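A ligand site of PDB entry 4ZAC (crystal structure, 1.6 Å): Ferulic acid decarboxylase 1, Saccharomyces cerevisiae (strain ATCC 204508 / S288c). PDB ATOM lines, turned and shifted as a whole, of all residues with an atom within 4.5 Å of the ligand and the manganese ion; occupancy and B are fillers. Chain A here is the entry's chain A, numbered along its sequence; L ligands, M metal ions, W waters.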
ATOM      1  N   GLN A 154      30.318  16.531 -25.793  1.00  0.00           N
ATOM      2  CA  GLN A 154      29.251  17.064 -24.923  1.00  0.00           C
ATOM      3  C   GLN A 154      28.247  15.925 -24.557  1.00  0.00           C
ATOM      4  O   GLN A 154      27.289  15.583 -25.320  1.00  0.00           O
ATOM      5  CB  GLN A 154      28.638  18.223 -25.646  1.00  0.00           C
ATOM      6  CG  GLN A 154      27.228  18.743 -25.279  1.00  0.00           C
ATOM      7  CD  GLN A 154      26.956  18.894 -23.779  1.00  0.00           C
ATOM      8  OE1 GLN A 154      27.691  18.357 -22.971  1.00  0.00           O
ATOM      9  NE2 GLN A 154      25.957  19.733 -23.425  1.00  0.00           N
ATOM     10  N   THR A 155      28.538  15.330 -23.371  1.00  0.00           N
ATOM     11  CA  THR A 155      27.527  14.462 -22.791  1.00  0.00           C
ATOM     12  C   THR A 155      27.134  14.903 -21.389  1.00  0.00           C
ATOM     13  O   THR A 155      26.181  14.361 -20.846  1.00  0.00           O
ATOM     14  CB  THR A 155      28.033  13.029 -22.692  1.00  0.00           C
ATOM     15  OG1 THR A 155      29.259  12.909 -21.894  1.00  0.00           O
ATOM     16  CG2 THR A 155      28.388  12.464 -24.136  1.00  0.00           C
ATOM     17  N   TYR A 156      27.937  15.770 -20.737  1.00  0.00           N
ATOM     18  CA  TYR A 156      27.568  16.169 -19.353  1.00  0.00           C
ATOM     19  C   TYR A 156      28.018  17.589 -19.065  1.00  0.00           C
ATOM     20  O   TYR A 156      28.479  17.962 -17.950  1.00  0.00           O
ATOM     21  CB  TYR A 156      28.185  15.162 -18.379  1.00  0.00           C
ATOM     22  CG  TYR A 156      27.483  15.108 -17.019  1.00  0.00           C
ATOM     23  CD1 TYR A 156      26.299  14.442 -16.903  1.00  0.00           C
ATOM     24  CD2 TYR A 156      28.055  15.729 -15.846  1.00  0.00           C
ATOM     25  CE1 TYR A 156      25.607  14.404 -15.692  1.00  0.00           C
ATOM     26  CE2 TYR A 156      27.407  15.591 -14.594  1.00  0.00           C
ATOM     27  CZ  TYR A 156      26.193  14.933 -14.557  1.00  0.00           C
ATOM     28  OH  TYR A 156      25.483  14.731 -13.390  1.00  0.00           O
ATOM     29  N   TRP A 168      15.189  35.469 -20.692  1.00  0.00           N
ATOM     30  CA  TRP A 168      15.174  33.964 -20.343  1.00  0.00           C
ATOM     31  C   TRP A 168      16.495  33.445 -20.782  1.00  0.00           C
ATOM     32  O   TRP A 168      16.894  33.484 -21.975  1.00  0.00           O
ATOM     33  CB  TRP A 168      14.001  33.284 -21.075  1.00  0.00           C
ATOM     34  CG  TRP A 168      13.958  31.749 -20.870  1.00  0.00           C
ATOM     35  CD1 TRP A 168      14.584  31.040 -19.873  1.00  0.00           C
ATOM     36  CD2 TRP A 168      13.281  30.819 -21.683  1.00  0.00           C
ATOM     37  NE1 TRP A 168      14.323  29.655 -20.068  1.00  0.00           N
ATOM     38  CE2 TRP A 168      13.515  29.528 -21.161  1.00  0.00           C
ATOM     39  CE3 TRP A 168      12.476  30.979 -22.830  1.00  0.00           C
ATOM     40  CZ2 TRP A 168      12.963  28.361 -21.746  1.00  0.00           C
ATOM     41  CZ3 TRP A 168      11.964  29.860 -23.475  1.00  0.00           C
ATOM     42  CH2 TRP A 168      12.200  28.549 -22.907  1.00  0.00           C
ATOM     43  N   ASN A 170      18.495  29.935 -20.756  1.00  0.00           N
ATOM     44  CA  ASN A 170      18.225  28.494 -20.456  1.00  0.00           C
ATOM     45  C   ASN A 170      19.536  27.724 -20.347  1.00  0.00           C
ATOM     46  O   ASN A 170      20.462  27.972 -21.095  1.00  0.00           O
ATOM     47  CB  ASN A 170      17.411  27.903 -21.646  1.00  0.00           C
ATOM     48  CG  ASN A 170      16.786  26.587 -21.337  1.00  0.00           C
ATOM     49  OD1 ASN A 170      17.336  25.457 -21.614  1.00  0.00           O
ATOM     50  ND2 ASN A 170      15.718  26.647 -20.664  1.00  0.00           N
ATOM     51  N   TRP A 171      19.614  26.852 -19.353  1.00  0.00           N
ATOM     52  CA  TRP A 171      20.724  25.924 -19.201  1.00  0.00           C
ATOM     53  C   TRP A 171      20.137  24.489 -19.408  1.00  0.00           C
ATOM     54  O   TRP A 171      19.222  24.066 -18.691  1.00  0.00           O
ATOM     55  CB  TRP A 171      21.233  26.014 -17.753  1.00  0.00           C
ATOM     56  CG  TRP A 171      21.913  27.311 -17.423  1.00  0.00           C
ATOM     57  CD1 TRP A 171      22.208  28.365 -18.303  1.00  0.00           C
ATOM     58  CD2 TRP A 171      22.467  27.665 -16.125  1.00  0.00           C
ATOM     59  NE1 TRP A 171      22.956  29.383 -17.589  1.00  0.00           N
ATOM     60  CE2 TRP A 171      23.061  28.966 -16.254  1.00  0.00           C
ATOM     61  CE3 TRP A 171      22.497  27.005 -14.888  1.00  0.00           C
ATOM     62  CZ2 TRP A 171      23.805  29.611 -15.164  1.00  0.00           C
ATOM     63  CZ3 TRP A 171      23.208  27.663 -13.794  1.00  0.00           C
ATOM     64  CH2 TRP A 171      23.802  28.971 -13.960  1.00  0.00           C
ATOM     65  N   SER A 172      20.787  23.746 -20.283  1.00  0.00           N
ATOM     66  CA  SER A 172      20.328  22.373 -20.604  1.00  0.00           C
ATOM     67  C   SER A 172      21.410  21.495 -21.144  1.00  0.00           C
ATOM     68  O   SER A 172      22.443  21.918 -21.588  1.00  0.00           O
ATOM     69  CB  SER A 172      19.080  22.454 -21.567  1.00  0.00           C
ATOM     70  OG  SER A 172      19.590  22.906 -22.765  1.00  0.00           O
ATOM     71  N   ILE A 173      21.196  20.200 -20.957  1.00  0.00           N
ATOM     72  CA  ILE A 173      22.100  19.194 -21.532  1.00  0.00           C
ATOM     73  C   ILE A 173      21.436  18.692 -22.860  1.00  0.00           C
ATOM     74  O   ILE A 173      20.284  18.333 -22.898  1.00  0.00           O
ATOM     75  CB  ILE A 173      22.294  18.016 -20.600  1.00  0.00           C
ATOM     76  CG1 ILE A 173      22.813  18.551 -19.223  1.00  0.00           C
ATOM     77  CG2 ILE A 173      23.362  17.002 -21.194  1.00  0.00           C
ATOM     78  CD1 ILE A 173      23.110  17.285 -18.268  1.00  0.00           C
ATOM     79  N   ALA A 174      22.260  18.671 -23.904  1.00  0.00           N
ATOM     80  CA  ALA A 174      21.875  17.981 -25.171  1.00  0.00           C
ATOM     81  C   ALA A 174      23.156  17.484 -25.770  1.00  0.00           C
ATOM     82  O   ALA A 174      24.225  18.132 -25.715  1.00  0.00           O
ATOM     83  CB  ALA A 174      21.245  18.970 -26.139  1.00  0.00           C
ATOM     84  N   ARG A 175      23.117  16.309 -26.369  1.00  0.00           N
ATOM     85  CA  ARG A 175      24.426  15.713 -26.792  1.00  0.00           C
ATOM     86  C   ARG A 175      25.043  16.529 -27.963  1.00  0.00           C
ATOM     87  O   ARG A 175      24.369  17.192 -28.695  1.00  0.00           O
ATOM     88  CB  ARG A 175      24.222  14.318 -27.344  1.00  0.00           C
ATOM     89  CG  ARG A 175      23.332  14.166 -28.640  1.00  0.00           C
ATOM     90  CD  ARG A 175      23.055  12.748 -28.846  1.00  0.00           C
ATOM     91  NE  ARG A 175      22.661  12.556 -30.285  1.00  0.00           N
ATOM     92  CZ  ARG A 175      21.835  11.585 -30.681  1.00  0.00           C
ATOM     93  NH1 ARG A 175      21.173  10.798 -29.810  1.00  0.00           N
ATOM     94  NH2 ARG A 175      21.572  11.492 -32.002  1.00  0.00           N
ATOM     95  N   LEU A 187      21.942  17.524 -30.949  1.00  0.00           N
ATOM     96  CA  LEU A 187      20.472  17.565 -31.011  1.00  0.00           C
ATOM     97  C   LEU A 187      19.946  18.943 -30.552  1.00  0.00           C
ATOM     98  O   LEU A 187      20.313  19.469 -29.448  1.00  0.00           O
ATOM     99  CB  LEU A 187      19.891  16.452 -30.151  1.00  0.00           C
ATOM    100  CG  LEU A 187      20.051  15.043 -30.727  1.00  0.00           C
ATOM    101  CD1 LEU A 187      19.461  14.004 -29.720  1.00  0.00           C
ATOM    102  CD2 LEU A 187      19.329  14.862 -32.092  1.00  0.00           C
ATOM    103  N   ILE A 189      16.251  19.876 -30.677  1.00  0.00           N
ATOM    104  CA  ILE A 189      14.943  19.319 -31.092  1.00  0.00           C
ATOM    105  C   ILE A 189      13.769  19.799 -30.307  1.00  0.00           C
ATOM    106  O   ILE A 189      13.876  19.996 -29.094  1.00  0.00           O
ATOM    107  CB  ILE A 189      14.931  17.765 -31.115  1.00  0.00           C
ATOM    108  CG1 ILE A 189      15.036  17.172 -29.670  1.00  0.00           C
ATOM    109  CG2 ILE A 189      16.003  17.269 -32.085  1.00  0.00           C
ATOM    110  CD1 ILE A 189      14.583  15.639 -29.483  1.00  0.00           C
ATOM    111  N   GLN A 192      12.308  20.719 -26.777  1.00  0.00           N
ATOM    112  CA  GLN A 192      13.343  21.179 -25.819  1.00  0.00           C
ATOM    113  C   GLN A 192      13.503  22.692 -25.849  1.00  0.00           C
ATOM    114  O   GLN A 192      13.357  23.349 -26.925  1.00  0.00           O
ATOM    115  CB  GLN A 192      14.688  20.515 -26.106  1.00  0.00           C
ATOM    116  CG  GLN A 192      14.521  18.891 -26.062  1.00  0.00           C
ATOM    117  CD  GLN A 192      14.160  18.449 -24.693  1.00  0.00           C
ATOM    118  OE1 GLN A 192      13.076  18.742 -24.088  1.00  0.00           O
ATOM    119  NE2 GLN A 192      15.157  17.785 -24.056  1.00  0.00           N
ATOM    120  N   HIS A 193      13.911  23.258 -24.689  1.00  0.00           N
ATOM    121  CA  HIS A 193      14.027  24.715 -24.672  1.00  0.00           C
ATOM    122  C   HIS A 193      15.186  25.227 -25.525  1.00  0.00           C
ATOM    123  O   HIS A 193      15.137  26.403 -25.927  1.00  0.00           O
ATOM    124  CB  HIS A 193      14.095  25.221 -23.221  1.00  0.00           C
ATOM    125  CG  HIS A 193      12.788  24.991 -22.512  1.00  0.00           C
ATOM    126  ND1 HIS A 193      12.720  24.957 -21.139  1.00  0.00           N
ATOM    127  CD2 HIS A 193      11.536  24.760 -22.988  1.00  0.00           C
ATOM    128  CE1 HIS A 193      11.445  24.744 -20.782  1.00  0.00           C
ATOM    129  NE2 HIS A 193      10.711  24.631 -21.892  1.00  0.00           N
ATOM    130  N   ILE A 194      16.233  24.472 -25.698  1.00  0.00           N
ATOM    131  CA  ILE A 194      17.348  24.966 -26.534  1.00  0.00           C
ATOM    132  C   ILE A 194      16.791  25.264 -27.968  1.00  0.00           C
ATOM    133  O   ILE A 194      17.171  26.209 -28.575  1.00  0.00           O
ATOM    134  CB  ILE A 194      18.506  23.931 -26.518  1.00  0.00           C
ATOM    135  CG1 ILE A 194      19.705  24.550 -27.242  1.00  0.00           C
ATOM    136  CG2 ILE A 194      17.973  22.544 -27.179  1.00  0.00           C
ATOM    137  CD1 ILE A 194      20.978  23.574 -27.026  1.00  0.00           C
ATOM    138  N   SER A 226      20.157  21.569 -15.276  1.00  0.00           N
ATOM    139  CA  SER A 226      20.263  21.527 -16.755  1.00  0.00           C
ATOM    140  C   SER A 226      19.480  20.327 -17.317  1.00  0.00           C
ATOM    141  O   SER A 226      18.943  20.452 -18.470  1.00  0.00           O
ATOM    142  CB  SER A 226      21.722  21.456 -17.209  1.00  0.00           C
ATOM    143  OG  SER A 226      22.279  22.768 -16.853  1.00  0.00           O
ATOM    144  N   SER A 227      19.415  19.189 -16.598  1.00  0.00           N
ATOM    145  CA  SER A 227      18.745  17.994 -17.067  1.00  0.00           C
ATOM    146  C   SER A 227      17.258  17.941 -16.677  1.00  0.00           C
ATOM    147  O   SER A 227      16.552  16.937 -16.943  1.00  0.00           O
ATOM    148  CB  SER A 227      19.389  16.742 -16.514  1.00  0.00           C
ATOM    149  OG  SER A 227      18.762  15.581 -17.009  1.00  0.00           O
ATOM    150  N   MET A 228      16.781  18.997 -16.016  1.00  0.00           N
ATOM    151  CA  MET A 228      15.405  18.986 -15.467  1.00  0.00           C
ATOM    152  C   MET A 228      14.440  19.838 -16.316  1.00  0.00           C
ATOM    153  O   MET A 228      14.811  20.962 -16.708  1.00  0.00           O
ATOM    154  CB  MET A 228      15.453  19.655 -14.087  1.00  0.00           C
ATOM    155  CG  MET A 228      14.097  19.501 -13.369  1.00  0.00           C
ATOM    156  SD  MET A 228      14.490  20.150 -11.630  1.00  0.00           S
ATOM    157  CE  MET A 228      12.953  19.766 -10.878  1.00  0.00           C
ATOM    158  N   PRO A 229      13.245  19.335 -16.597  1.00  0.00           N
ATOM    159  CA  PRO A 229      12.304  20.064 -17.435  1.00  0.00           C
ATOM    160  C   PRO A 229      11.489  21.034 -16.598  1.00  0.00           C
ATOM    161  O   PRO A 229      10.291  20.809 -16.415  1.00  0.00           O
ATOM    162  CB  PRO A 229      11.491  18.939 -18.097  1.00  0.00           C
ATOM    163  CG  PRO A 229      11.419  17.824 -16.955  1.00  0.00           C
ATOM    164  CD  PRO A 229      12.844  17.905 -16.385  1.00  0.00           C
ATOM    165  N   ILE A 230      12.143  22.105 -16.138  1.00  0.00           N
ATOM    166  CA  ILE A 230      11.388  23.143 -15.412  1.00  0.00           C
ATOM    167  C   ILE A 230      10.629  23.981 -16.462  1.00  0.00           C
ATOM    168  O   ILE A 230      10.812  23.810 -17.655  1.00  0.00           O
ATOM    169  CB  ILE A 230      12.344  24.006 -14.555  1.00  0.00           C
ATOM    170  CG1 ILE A 230      13.263  24.878 -15.429  1.00  0.00           C
ATOM    171  CG2 ILE A 230      13.171  23.098 -13.660  1.00  0.00           C
ATOM    172  CD1 ILE A 230      14.081  25.887 -14.498  1.00  0.00           C
ATOM    173  N   GLU A 236      17.071  28.573 -15.503  1.00  0.00           N
ATOM    174  CA  GLU A 236      17.553  27.513 -14.578  1.00  0.00           C
ATOM    175  C   GLU A 236      18.423  28.189 -13.490  1.00  0.00           C
ATOM    176  O   GLU A 236      18.393  27.755 -12.353  1.00  0.00           O
ATOM    177  CB  GLU A 236      18.407  26.462 -15.323  1.00  0.00           C
ATOM    178  CG  GLU A 236      17.523  25.360 -16.093  1.00  0.00           C
ATOM    179  CD  GLU A 236      16.828  25.857 -17.370  1.00  0.00           C
ATOM    180  OE1 GLU A 236      17.143  26.991 -17.858  1.00  0.00           O
ATOM    181  OE2 GLU A 236      16.030  25.028 -17.884  1.00  0.00           O
ATOM    182  N   PHE A 283      24.168   7.768 -31.798  1.00  0.00           N
ATOM    183  CA  PHE A 283      24.854   7.797 -30.513  1.00  0.00           C
ATOM    184  C   PHE A 283      24.177   6.788 -29.611  1.00  0.00           C
ATOM    185  O   PHE A 283      22.938   6.672 -29.655  1.00  0.00           O
ATOM    186  CB  PHE A 283      24.649   9.182 -29.906  1.00  0.00           C
ATOM    187  CG  PHE A 283      25.397   9.357 -28.565  1.00  0.00           C
ATOM    188  CD1 PHE A 283      26.790   9.107 -28.458  1.00  0.00           C
ATOM    189  CD2 PHE A 283      24.650   9.784 -27.406  1.00  0.00           C
ATOM    190  CE1 PHE A 283      27.472   9.245 -27.166  1.00  0.00           C
ATOM    191  CE2 PHE A 283      25.346   9.952 -26.170  1.00  0.00           C
ATOM    192  CZ  PHE A 283      26.693   9.676 -26.032  1.00  0.00           C
ATOM    193  N   GLU A 285      22.322   5.381 -26.840  1.00  0.00           N
ATOM    194  CA  GLU A 285      21.384   6.242 -26.119  1.00  0.00           C
ATOM    195  C   GLU A 285      20.734   5.515 -24.843  1.00  0.00           C
ATOM    196  O   GLU A 285      21.057   4.375 -24.498  1.00  0.00           O
ATOM    197  CB  GLU A 285      20.350   6.669 -27.109  1.00  0.00           C
ATOM    198  CG  GLU A 285      20.586   8.068 -27.671  1.00  0.00           C
ATOM    199  CD  GLU A 285      20.557   9.211 -26.587  1.00  0.00           C
ATOM    200  OE1 GLU A 285      20.171   8.979 -25.338  1.00  0.00           O
ATOM    201  OE2 GLU A 285      20.903  10.429 -26.998  1.00  0.00           O
ATOM    202  N   SER A 317      29.079  11.291 -19.530  1.00  0.00           N
ATOM    203  CA  SER A 317      28.071  10.228 -19.325  1.00  0.00           C
ATOM    204  C   SER A 317      28.079   9.362 -20.646  1.00  0.00           C
ATOM    205  O   SER A 317      28.169   9.842 -21.754  1.00  0.00           O
ATOM    206  CB  SER A 317      26.655  10.899 -19.256  1.00  0.00           C
ATOM    207  OG  SER A 317      25.624   9.943 -19.214  1.00  0.00           O
ATOM    208  N   PRO A 319      25.765   6.638 -22.105  1.00  0.00           N
ATOM    209  CA  PRO A 319      24.426   6.028 -21.899  1.00  0.00           C
ATOM    210  C   PRO A 319      24.347   4.649 -22.469  1.00  0.00           C
ATOM    211  O   PRO A 319      25.033   4.253 -23.437  1.00  0.00           O
ATOM    212  CB  PRO A 319      23.431   6.980 -22.710  1.00  0.00           C
ATOM    213  CG  PRO A 319      24.238   8.277 -22.843  1.00  0.00           C
ATOM    214  CD  PRO A 319      25.731   7.816 -22.957  1.00  0.00           C
ATOM    215  N   GLU A 325      23.314   8.188 -16.084  1.00  0.00           N
ATOM    216  CA  GLU A 325      22.680   9.479 -15.878  1.00  0.00           C
ATOM    217  C   GLU A 325      21.369   9.645 -16.647  1.00  0.00           C
ATOM    218  O   GLU A 325      20.583  10.501 -16.317  1.00  0.00           O
ATOM    219  CB  GLU A 325      23.610  10.618 -16.236  1.00  0.00           C
ATOM    220  CG  GLU A 325      24.939  10.718 -15.397  1.00  0.00           C
ATOM    221  CD  GLU A 325      25.929   9.610 -15.593  1.00  0.00           C
ATOM    222  OE1 GLU A 325      25.960   8.958 -16.662  1.00  0.00           O
ATOM    223  OE2 GLU A 325      26.726   9.399 -14.679  1.00  0.00           O
ATOM    224  N   THR A 326      21.257   8.925 -17.788  1.00  0.00           N
ATOM    225  CA  THR A 326      20.000   9.114 -18.555  1.00  0.00           C
ATOM    226  C   THR A 326      18.855   8.427 -17.827  1.00  0.00           C
ATOM    227  O   THR A 326      17.729   8.560 -18.267  1.00  0.00           O
ATOM    228  CB  THR A 326      20.136   8.595 -19.992  1.00  0.00           C
ATOM    229  OG1 THR A 326      20.341   7.165 -20.002  1.00  0.00           O
ATOM    230  CG2 THR A 326      21.279   9.254 -20.686  1.00  0.00           C
ATOM    231  N   LEU A 329      19.170  10.850 -13.781  1.00  0.00           N
ATOM    232  CA  LEU A 329      18.864  12.271 -13.849  1.00  0.00           C
ATOM    233  C   LEU A 329      17.671  12.420 -14.812  1.00  0.00           C
ATOM    234  O   LEU A 329      16.630  12.982 -14.394  1.00  0.00           O
ATOM    235  CB  LEU A 329      19.998  13.115 -14.365  1.00  0.00           C
ATOM    236  CG  LEU A 329      21.192  13.093 -13.434  1.00  0.00           C
ATOM    237  CD1 LEU A 329      22.236  14.039 -14.019  1.00  0.00           C
ATOM    238  CD2 LEU A 329      20.862  13.580 -11.978  1.00  0.00           C
ATOM    239  N   ILE A 330      17.680  11.906 -16.037  1.00  0.00           N
ATOM    240  CA  ILE A 330      16.599  12.268 -16.913  1.00  0.00           C
ATOM    241  C   ILE A 330      15.277  11.731 -16.303  1.00  0.00           C
ATOM    242  O   ILE A 330      14.320  12.430 -16.181  1.00  0.00           O
ATOM    243  CB  ILE A 330      16.787  11.659 -18.325  1.00  0.00           C
ATOM    244  CG1 ILE A 330      18.021  12.368 -18.961  1.00  0.00           C
ATOM    245  CG2 ILE A 330      15.551  12.058 -19.263  1.00  0.00           C
ATOM    246  CD1 ILE A 330      18.281  11.807 -20.366  1.00  0.00           C
ATOM    247  N   LYS A 394       5.159  18.592 -22.289  1.00  0.00           N
ATOM    248  CA  LYS A 394       6.585  18.352 -22.499  1.00  0.00           C
ATOM    249  C   LYS A 394       7.083  17.343 -21.387  1.00  0.00           C
ATOM    250  O   LYS A 394       7.952  16.548 -21.662  1.00  0.00           O
ATOM    251  CB  LYS A 394       7.327  19.695 -22.354  1.00  0.00           C
ATOM    252  CG  LYS A 394       8.901  19.541 -22.409  1.00  0.00           C
ATOM    253  CD  LYS A 394       9.439  20.984 -22.625  1.00  0.00           C
ATOM    254  CE  LYS A 394      11.014  21.051 -22.594  1.00  0.00           C
ATOM    255  NZ  LYS A 394      11.521  20.686 -21.190  1.00  0.00           N
HETATM  256  C1  LIG L   1      20.169  14.617 -20.281  1.00  0.00           C
HETATM  257  C2  LIG L   1      21.292  13.969 -19.758  1.00  0.00           C
HETATM  258  C3  LIG L   1      22.301  13.345 -20.512  1.00  0.00           C
HETATM  259  C4  LIG L   1      18.948  15.381 -23.623  1.00  0.00           C
HETATM  260  C5  LIG L   1      22.144  13.286 -21.923  1.00  0.00           C
HETATM  261  N1  LIG L   1      19.034  16.030 -26.259  1.00  0.00           N
HETATM  262  C6  LIG L   1      18.030  16.481 -25.543  1.00  0.00           C
HETATM  263  C7  LIG L   1      24.157  11.703 -22.275  1.00  0.00           C
HETATM  264  C8  LIG L   1      23.078  12.712 -22.867  1.00  0.00           C
HETATM  265  C9  LIG L   1      21.640  13.101 -24.529  1.00  0.00           C
HETATM  266  O1  LIG L   1      17.340  17.318 -26.054  1.00  0.00           O
HETATM  267  N2  LIG L   1      17.986  16.213 -24.189  1.00  0.00           N
HETATM  268  C10 LIG L   1      19.951  15.115 -25.732  1.00  0.00           C
HETATM  269  O2  LIG L   1      20.808  14.803 -26.552  1.00  0.00           O
HETATM  270  C11 LIG L   1      19.954  14.796 -24.390  1.00  0.00           C
HETATM  271  N3  LIG L   1      20.831  13.902 -23.785  1.00  0.00           N
HETATM  272  C12 LIG L   1      22.223  11.937 -23.836  1.00  0.00           C
HETATM  273  C13 LIG L   1      23.967  13.802 -23.524  1.00  0.00           C
HETATM  274  C14 LIG L   1      20.973  13.919 -22.412  1.00  0.00           C
HETATM  275  C15 LIG L   1      23.527  12.700 -19.754  1.00  0.00           C
HETATM  276  C16 LIG L   1      21.347  13.993 -18.231  1.00  0.00           C
HETATM  277  C17 LIG L   1      20.022  14.609 -21.674  1.00  0.00           C
HETATM  278  N4  LIG L   1      18.870  15.147 -22.311  1.00  0.00           N
HETATM  279  C18 LIG L   1      17.781  15.618 -21.467  1.00  0.00           C
HETATM  280  C19 LIG L   1      17.574  17.127 -21.195  1.00  0.00           C
HETATM  281  O3  LIG L   1      18.776  17.638 -20.640  1.00  0.00           O
HETATM  282  C20 LIG L   1      16.320  17.403 -20.521  1.00  0.00           C
HETATM  283  O4  LIG L   1      15.155  16.913 -21.220  1.00  0.00           O
HETATM  284  C21 LIG L   1      16.190  18.808 -19.944  1.00  0.00           C
HETATM  285  O5  LIG L   1      14.891  18.927 -19.369  1.00  0.00           O
HETATM  286  C22 LIG L   1      16.299  19.699 -21.218  1.00  0.00           C
HETATM  287  O6  LIG L   1      16.266  21.076 -20.676  1.00  0.00           O
HETATM  288  P1  LIG L   1      15.061  22.090 -21.057  1.00  0.00           P
HETATM  289  O7  LIG L   1      14.908  22.024 -22.567  1.00  0.00           O
HETATM  290  O8  LIG L   1      13.877  21.614 -20.291  1.00  0.00           O
HETATM  291  O9  LIG L   1      15.508  23.443 -20.532  1.00  0.00           O
HETATM  292 MN    MN M   1      14.529  25.148 -19.489  1.00  0.00          MN
HETATM  293  O   HOH W   1      12.433  18.093 -21.590  1.00  0.00           O
HETATM  294  O   HOH W   2      18.108  19.531 -24.415  1.00  0.00           O
HETATM  295  O   HOH W   3      17.063  22.160 -23.989  1.00  0.00           O
HETATM  296  O   HOH W   4      13.369  23.453 -18.432  1.00  0.00           O
HETATM  297  O   HOH W   5      17.725  19.023 -28.258  1.00  0.00           O
HETATM  298  O   HOH W   6      13.746  15.204 -19.975  1.00  0.00           O
HETATM  299  O   HOH W   7      13.240  26.773 -18.478  1.00  0.00           O
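O5 of the ligand sits close to O of Met 228 (3.4 Å).
The side-chain amide nitrogen of Gln 192 lies within hydrogen-bond range of an oxygen (O4) of the ligand.
The backbone carbonyl oxygen (O) of Ile 173 is in hydrogen-bond range of an oxygen (O3) of the ligand (2.8 Å).
O7 of the ligand sits at hydrogen-bond distance from N of His 193 (2.6 Å).
O8 of the ligand is in salt-bridge range of NZ of Lys 394 (2.7 Å).
N of Arg 175 is in hydrogen-bond range of O2 of the ligand, 2.8 Å away.
The side-chain carboxylate of Glu 325 lies within hydrogen-bond range of the side-chain hydroxyl of Ser 317 (2.8 Å).
The backbone carbonyl oxygen (O) of Arg 175 is in hydrogen-bond range of the backbone NH (N) of Leu 187 (3.3 Å).
The guanidinium group (NH1) of Arg 175 lies within salt-bridge range of the side-chain carboxylate (OE2) of Glu 285.
O of Ser 226 lies within hydrogen-bond range of N of Ile 173 (3.4 Å).
The side-chain amide nitrogen (ND2) of Asn 170 lies close to the indole nitrogen (NE1) of Trp 168 (3.4 Å).
O of Ala 174 lies close to NE2 of Gln 154 (3.3 Å).
The side-chain carboxylate of Glu 236 is in hydrogen-bond range of the backbone NH of Trp 171, 2.9 Å away.
The side-chain hydroxyl (OG1) of Thr 155 sits at hydrogen-bond distance from the backbone NH (N) of Ser 317 (2.9 Å).
The backbone nitrogen (N) of Pro 229 lies close to an oxygen (O5) of the ligand.
Merely in contact with the ligand: Ser 172 (3.3 Å), Ser 227 (3.3 Å), Thr 155 (3.3 Å), Ile 330 (3.4 Å), Pro 319 (3.5 Å), Ala 174 (3.5 Å), Ser 317 (3.5 Å), Ser 226 (3.5 Å), Leu 187 (3.5 Å) and Glu 285 (3.7 Å).
Within 4 Å of the ligand: Thr 155, Asn 170, Ser 172, Ile 173, Ala 174, Arg 175, Leu 187, Gln 192, His 193, Ser 226, Ser 227, Met 228, Pro 229, Glu 236, Glu 285, Ser 317, Pro 319, Ile 330 and Lys 394.
The nearest printed residue that does not touch the manganese ion is Trp 168 (4.2 Å).
The manganese ion is bound by the side-chain carboxylate of Glu 236 (2.2 Å), an oxygen (O9) of the ligand (2.2 Å), the side-chain amide nitrogen of Asn 170 (2.2 Å), water W7 (2.3 Å), water W4 (2.3 Å) and a ring nitrogen (ND1) of His 193 (2.5 Å).
The manganese ion has six donor atoms within binding distance.
Water W4 lies within hydrogen-bond range of O8 of the ligand, O of Ile 230 and O of Met 228.
Water W3 lies within hydrogen-bond range of O7 of the ligand, OG of Ser 172, N of Ile 194 and N of His 193.
Water W5 lies within hydrogen-bond range of O1 of the ligand (2.8 Å), O of Leu 187 (2.9 Å) and N of Ile 189 (3.0 Å).
Water W2 lies within hydrogen-bond range of an oxygen (O1) of the ligand (2.9 Å), the backbone carbonyl oxygen of Ile 173 (2.9 Å) and the side-chain amide nitrogen of Gln 192 (3.4 Å).
Water W1 lies within hydrogen-bond range of the side-chain amide oxygen (OE1) of Gln 192 (2.7 Å), the side-chain amino group (NZ) of Lys 394 (2.8 Å) and an oxygen (O4) of the ligand (3.0 Å).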
